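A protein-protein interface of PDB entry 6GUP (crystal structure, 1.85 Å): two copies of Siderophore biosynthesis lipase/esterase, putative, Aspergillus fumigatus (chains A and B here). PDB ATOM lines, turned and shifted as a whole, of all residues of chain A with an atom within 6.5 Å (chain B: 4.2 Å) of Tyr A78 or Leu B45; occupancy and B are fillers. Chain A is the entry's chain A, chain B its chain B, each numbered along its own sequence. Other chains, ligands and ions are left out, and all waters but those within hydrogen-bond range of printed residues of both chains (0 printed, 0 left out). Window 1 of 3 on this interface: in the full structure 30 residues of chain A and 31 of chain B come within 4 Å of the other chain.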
ATOM      1  N   THR A  22      37.254  22.269   8.750  1.00  0.00           N
ATOM      2  CA  THR A  22      36.077  21.962   9.574  1.00  0.00           C
ATOM      3  C   THR A  22      34.738  22.233   8.870  1.00  0.00           C
ATOM      4  O   THR A  22      33.757  21.532   9.132  1.00  0.00           O
ATOM      5  CB  THR A  22      36.116  22.783  10.885  1.00  0.00           C
ATOM      6  OG1 THR A  22      37.373  22.578  11.542  1.00  0.00           O
ATOM      7  CG2 THR A  22      34.984  22.386  11.839  1.00  0.00           C
ATOM      8  N   LEU A  23      34.695  23.239   7.994  1.00  0.00           N
ATOM      9  CA  LEU A  23      33.431  23.758   7.454  1.00  0.00           C
ATOM     10  C   LEU A  23      33.244  23.422   5.976  1.00  0.00           C
ATOM     11  O   LEU A  23      34.208  23.425   5.204  1.00  0.00           O
ATOM     12  CB  LEU A  23      33.358  25.274   7.670  1.00  0.00           C
ATOM     13  CG  LEU A  23      33.512  25.733   9.129  1.00  0.00           C
ATOM     14  CD1 LEU A  23      33.731  27.236   9.219  1.00  0.00           C
ATOM     15  CD2 LEU A  23      32.310  25.314   9.964  1.00  0.00           C
ATOM     16  N   VAL A  24      31.993  23.150   5.596  1.00  0.00           N
ATOM     17  CA  VAL A  24      31.650  22.698   4.242  1.00  0.00           C
ATOM     18  C   VAL A  24      30.639  23.608   3.556  1.00  0.00           C
ATOM     19  O   VAL A  24      29.880  24.327   4.214  1.00  0.00           O
ATOM     20  CB  VAL A  24      31.099  21.245   4.222  1.00  0.00           C
ATOM     21  CG1 VAL A  24      32.169  20.267   4.679  1.00  0.00           C
ATOM     22  CG2 VAL A  24      29.835  21.088   5.066  1.00  0.00           C
ATOM     23  N   GLY A  46      21.513  28.083  12.915  1.00  0.00           N
ATOM     24  CA  GLY A  46      21.404  26.670  13.272  1.00  0.00           C
ATOM     25  C   GLY A  46      20.895  25.742  12.175  1.00  0.00           C
ATOM     26  O   GLY A  46      20.586  24.582  12.455  1.00  0.00           O
ATOM     27  N   GLY A  48      22.550  25.119   8.873  1.00  0.00           N
ATOM     28  CA  GLY A  48      23.622  24.401   8.178  1.00  0.00           C
ATOM     29  C   GLY A  48      23.220  24.145   6.736  1.00  0.00           C
ATOM     30  O   GLY A  48      22.837  25.078   6.027  1.00  0.00           O
ATOM     31  N   THR A  73      27.755  25.478   5.938  1.00  0.00           N
ATOM     32  CA  THR A  73      27.785  25.388   7.390  1.00  0.00           C
ATOM     33  C   THR A  73      28.697  26.472   7.945  1.00  0.00           C
ATOM     34  O   THR A  73      29.704  26.831   7.327  1.00  0.00           O
ATOM     35  CB  THR A  73      28.309  24.022   7.875  1.00  0.00           C
ATOM     36  OG1 THR A  73      29.635  23.797   7.375  1.00  0.00           O
ATOM     37  CG2 THR A  73      27.392  22.901   7.416  1.00  0.00           C
ATOM     38  N   LEU A  74      28.320  26.989   9.110  1.00  0.00           N
ATOM     39  CA  LEU A  74      29.128  27.917   9.886  1.00  0.00           C
ATOM     40  C   LEU A  74      29.379  27.249  11.236  1.00  0.00           C
ATOM     41  O   LEU A  74      28.876  26.150  11.486  1.00  0.00           O
ATOM     42  CB  LEU A  74      28.371  29.238  10.069  1.00  0.00           C
ATOM     43  CG  LEU A  74      27.821  29.909   8.801  1.00  0.00           C
ATOM     44  CD1 LEU A  74      26.819  30.999   9.151  1.00  0.00           C
ATOM     45  CD2 LEU A  74      28.947  30.472   7.946  1.00  0.00           C
ATOM     46  N   THR A  75      30.151  27.897  12.103  1.00  0.00           N
ATOM     47  CA  THR A  75      30.288  27.445  13.493  1.00  0.00           C
ATOM     48  C   THR A  75      28.957  27.648  14.227  1.00  0.00           C
ATOM     49  O   THR A  75      28.580  26.836  15.074  1.00  0.00           O
ATOM     50  CB  THR A  75      31.420  28.194  14.229  1.00  0.00           C
ATOM     51  OG1 THR A  75      32.656  27.997  13.532  1.00  0.00           O
ATOM     52  CG2 THR A  75      31.576  27.698  15.674  1.00  0.00           C
ATOM     53  N   SER A  76      28.252  28.726  13.883  1.00  0.00           N
ATOM     54  CA  SER A  76      26.929  29.019  14.438  1.00  0.00           C
ATOM     55  C   SER A  76      25.825  28.040  14.013  1.00  0.00           C
ATOM     56  O   SER A  76      24.772  27.993  14.655  1.00  0.00           O
ATOM     57  CB  SER A  76      26.518  30.443  14.073  1.00  0.00           C
ATOM     58  OG  SER A  76      27.459  31.367  14.579  1.00  0.00           O
ATOM     59  N   SER A  77      26.049  27.290  12.932  1.00  0.00           N
ATOM     60  CA  SER A  77      25.195  26.146  12.582  1.00  0.00           C
ATOM     61  C   SER A  77      25.146  25.125  13.720  1.00  0.00           C
ATOM     62  O   SER A  77      24.082  24.595  14.037  1.00  0.00           O
ATOM     63  CB  SER A  77      25.689  25.453  11.307  1.00  0.00           C
ATOM     64  OG  SER A  77      25.843  26.375  10.241  1.00  0.00           O
ATOM     65  N   TYR A  78      26.305  24.871  14.327  1.00  0.00           N
ATOM     66  CA  TYR A  78      26.438  23.913  15.429  1.00  0.00           C
ATOM     67  C   TYR A  78      26.276  24.574  16.809  1.00  0.00           C
ATOM     68  O   TYR A  78      25.773  23.940  17.737  1.00  0.00           O
ATOM     69  CB  TYR A  78      27.778  23.176  15.317  1.00  0.00           C
ATOM     70  CG  TYR A  78      28.009  22.551  13.950  1.00  0.00           C
ATOM     71  CD1 TYR A  78      27.364  21.370  13.580  1.00  0.00           C
ATOM     72  CD2 TYR A  78      28.861  23.150  13.018  1.00  0.00           C
ATOM     73  CE1 TYR A  78      27.563  20.797  12.332  1.00  0.00           C
ATOM     74  CE2 TYR A  78      29.067  22.583  11.765  1.00  0.00           C
ATOM     75  CZ  TYR A  78      28.417  21.407  11.427  1.00  0.00           C
ATOM     76  OH  TYR A  78      28.613  20.835  10.191  1.00  0.00           O
ATOM     77  N   GLN A  79      26.683  25.838  16.939  1.00  0.00           N
ATOM     78  CA  GLN A  79      26.486  26.606  18.177  1.00  0.00           C
ATOM     79  C   GLN A  79      25.428  27.689  17.945  1.00  0.00           C
ATOM     80  O   GLN A  79      25.736  28.882  17.865  1.00  0.00           O
ATOM     81  CB  GLN A  79      27.808  27.220  18.664  1.00  0.00           C
ATOM     82  CG  GLN A  79      29.023  26.311  18.531  1.00  0.00           C
ATOM     83  CD  GLN A  79      30.237  26.817  19.293  1.00  0.00           C
ATOM     84  OE1 GLN A  79      30.117  27.521  20.298  1.00  0.00           O
ATOM     85  NE2 GLN A  79      31.422  26.450  18.819  1.00  0.00           N
ATOM     86  N   SER A  80      24.173  27.256  17.847  1.00  0.00           N
ATOM     87  CA  SER A  80      23.043  28.156  17.571  1.00  0.00           C
ATOM     88  C   SER A  80      22.467  28.877  18.805  1.00  0.00           C
ATOM     89  O   SER A  80      21.558  29.700  18.671  1.00  0.00           O
ATOM     90  CB  SER A  80      21.927  27.372  16.877  1.00  0.00           C
ATOM     91  OG  SER A  80      21.481  26.298  17.687  1.00  0.00           O
ATOM     92  N   TRP A  81      23.014  28.588  19.987  1.00  0.00           N
ATOM     93  CA  TRP A  81      22.488  29.092  21.270  1.00  0.00           C
ATOM     94  C   TRP A  81      23.240  30.314  21.809  1.00  0.00           C
ATOM     95  O   TRP A  81      22.783  30.916  22.773  1.00  0.00           O
ATOM     96  CB  TRP A  81      22.472  27.976  22.341  1.00  0.00           C
ATOM     97  CG  TRP A  81      23.586  27.000  22.198  1.00  0.00           C
ATOM     98  CD1 TRP A  81      23.522  25.777  21.597  1.00  0.00           C
ATOM     99  CD2 TRP A  81      24.946  27.181  22.602  1.00  0.00           C
ATOM    100  NE1 TRP A  81      24.753  25.175  21.619  1.00  0.00           N
ATOM    101  CE2 TRP A  81      25.648  26.013  22.231  1.00  0.00           C
ATOM    102  CE3 TRP A  81      25.639  28.212  23.253  1.00  0.00           C
ATOM    103  CZ2 TRP A  81      27.013  25.845  22.487  1.00  0.00           C
ATOM    104  CZ3 TRP A  81      27.000  28.044  23.511  1.00  0.00           C
ATOM    105  CH2 TRP A  81      27.670  26.868  23.123  1.00  0.00           C
ATOM    106  N   GLY B  44      30.886  11.861  15.795  1.00  0.00           N
ATOM    107  CA  GLY B  44      30.570  13.123  16.468  1.00  0.00           C
ATOM    108  C   GLY B  44      30.994  14.304  15.608  1.00  0.00           C
ATOM    109  O   GLY B  44      31.515  14.111  14.505  1.00  0.00           O
ATOM    110  N   LEU B  45      30.779  15.524  16.098  1.00  0.00           N
ATOM    111  CA  LEU B  45      31.134  16.727  15.334  1.00  0.00           C
ATOM    112  C   LEU B  45      32.634  16.749  15.035  1.00  0.00           C
ATOM    113  O   LEU B  45      33.455  16.730  15.955  1.00  0.00           O
ATOM    114  CB  LEU B  45      30.725  18.009  16.074  1.00  0.00           C
ATOM    115  CG  LEU B  45      31.068  19.339  15.381  1.00  0.00           C
ATOM    116  CD1 LEU B  45      30.419  19.440  14.006  1.00  0.00           C
ATOM    117  CD2 LEU B  45      30.659  20.522  16.243  1.00  0.00           C
ATOM    118  N   GLY B  46      32.970  16.780  13.744  1.00  0.00           N
ATOM    119  CA  GLY B  46      34.351  16.639  13.274  1.00  0.00           C
ATOM    120  C   GLY B  46      34.681  15.253  12.734  1.00  0.00           C
ATOM    121  O   GLY B  46      35.648  15.101  11.985  1.00  0.00           O
ATOM    122  N   ASP B  47      33.888  14.248  13.119  1.00  0.00           N
ATOM    123  CA  ASP B  47      34.046  12.863  12.665  1.00  0.00           C
ATOM    124  C   ASP B  47      32.907  12.391  11.744  1.00  0.00           C
ATOM    125  O   ASP B  47      32.883  11.221  11.353  1.00  0.00           O
ATOM    126  CB  ASP B  47      34.121  11.929  13.883  1.00  0.00           C
ATOM    127  CG  ASP B  47      35.247  12.292  14.847  1.00  0.00           C
ATOM    128  OD1 ASP B  47      36.276  12.845  14.403  1.00  0.00           O
ATOM    129  OD2 ASP B  47      35.101  12.012  16.056  1.00  0.00           O
ATOM    130  N   ALA B  50      31.074  16.525   8.049  1.00  0.00           N
ATOM    131  CA  ALA B  50      32.137  17.504   7.807  1.00  0.00           C
ATOM    132  C   ALA B  50      33.531  17.027   8.240  1.00  0.00           C
ATOM    133  O   ALA B  50      34.418  17.854   8.464  1.00  0.00           O
ATOM    134  CB  ALA B  50      31.791  18.806   8.512  1.00  0.00           C
ATOM    135  N   SER B  77      25.296  16.140  16.518  1.00  0.00           N
ATOM    136  CA  SER B  77      26.286  16.838  15.683  1.00  0.00           C
ATOM    137  C   SER B  77      26.162  18.344  15.854  1.00  0.00           C
ATOM    138  O   SER B  77      27.179  19.039  15.918  1.00  0.00           O
ATOM    139  CB  SER B  77      26.165  16.475  14.204  1.00  0.00           C
ATOM    140  OG  SER B  77      24.866  16.736  13.706  1.00  0.00           O
ATOM    141  N   TYR B  78      24.928  18.845  15.925  1.00  0.00           N
ATOM    142  CA  TYR B  78      24.699  20.256  16.237  1.00  0.00           C
ATOM    143  C   TYR B  78      25.168  20.564  17.658  1.00  0.00           C
ATOM    144  O   TYR B  78      26.118  21.326  17.832  1.00  0.00           O
ATOM    145  CB  TYR B  78      23.239  20.666  16.002  1.00  0.00           C
ATOM    146  CG  TYR B  78      22.864  20.733  14.529  1.00  0.00           C
ATOM    147  CD1 TYR B  78      23.609  21.505  13.632  1.00  0.00           C
ATOM    148  CD2 TYR B  78      21.763  20.034  14.030  1.00  0.00           C
ATOM    149  CE1 TYR B  78      23.278  21.572  12.287  1.00  0.00           C
ATOM    150  CE2 TYR B  78      21.422  20.097  12.684  1.00  0.00           C
ATOM    151  CZ  TYR B  78      22.182  20.867  11.817  1.00  0.00           C
ATOM    152  OH  TYR B  78      21.848  20.933  10.483  1.00  0.00           O
ATOM    153  N   SER B  80      26.953  18.727  19.653  1.00  0.00           N
ATOM    154  CA  SER B  80      28.290  18.137  19.869  1.00  0.00           C
ATOM    155  C   SER B  80      28.292  17.274  21.127  1.00  0.00           C
ATOM    156  O   SER B  80      27.454  16.385  21.279  1.00  0.00           O
ATOM    157  CB  SER B  80      29.418  19.174  19.920  1.00  0.00           C
ATOM    158  OG  SER B  80      29.220  20.209  18.973  1.00  0.00           O
ATOM    159  N   THR B 227      35.372  19.419  21.466  1.00  0.00           N
ATOM    160  CA  THR B 227      33.955  19.798  21.374  1.00  0.00           C
ATOM    161  C   THR B 227      33.488  20.364  22.720  1.00  0.00           C
ATOM    162  O   THR B 227      34.058  20.017  23.757  1.00  0.00           O
ATOM    163  CB  THR B 227      33.062  18.598  20.992  1.00  0.00           C
ATOM    164  OG1 THR B 227      33.396  17.463  21.799  1.00  0.00           O
ATOM    165  CG2 THR B 227      33.241  18.238  19.525  1.00  0.00           C
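The backbone carbonyl oxygen (O) of Tyr A78 sits close to the backbone carbonyl oxygen (O) of Tyr B78, 2.6 Å away.
Of the printed residues of chain B, Thr A22 touches Ala B50. Of chain B, only Leu B45 (3.6 Å), Ser B77 (3.3 Å) and Tyr B78 (2.6 Å) come within 4 Å of Tyr A78. Of chain A, only Tyr A78 (3.6 Å) comes within 4 Å of Leu B45. Printed residues of chain A within 4 Å of Ala B50: Thr A22. Printed residues of chain A within 4 Å of Tyr B78: Ser A77 and Tyr A78. The nearest residue of chain B that does not touch Tyr A78 is Ala B50 (4.1 Å).
Of the 9 printed residues of chain B, 4 touch a printed residue of chain A. Hydrophobic or aromatic side chains of chain B that line the printed part of chain A: Leu B45, Ala B50 and Tyr B78. Of the 14 printed residues of chain A, 3 touch a printed residue of chain B. Hydrophobic or aromatic side chains of chain A within 4 Å of the printed part of chain B: Tyr A78. Among the printed residues, no Asp or Glu carboxylate lies within 4 Å of a Lys or Arg side-chain nitrogen of the other chain.
The backbone NH (N) of Leu A74 sits at hydrogen-bond distance from the side-chain hydroxyl (OG) of Ser A77, 2.8 Å away. The backbone carbonyl oxygen (O) of Tyr B78 sits at hydrogen-bond distance from the side-chain hydroxyl (OG) of Ser B80, at 3.5 Å.
Ser A77 touches Tyr B78, and with the chains exchanged Tyr A78 touches Ser B77. Tyr A78 touches its own counterpart, Tyr B78. 4 positions are printed for both chains.
Among the printed residues, merely in contact across the chains: Thr A22 with Ala B50, Ser A77 with Tyr B78, Tyr A78 with Leu B45 and Tyr A78 with Ser B77.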
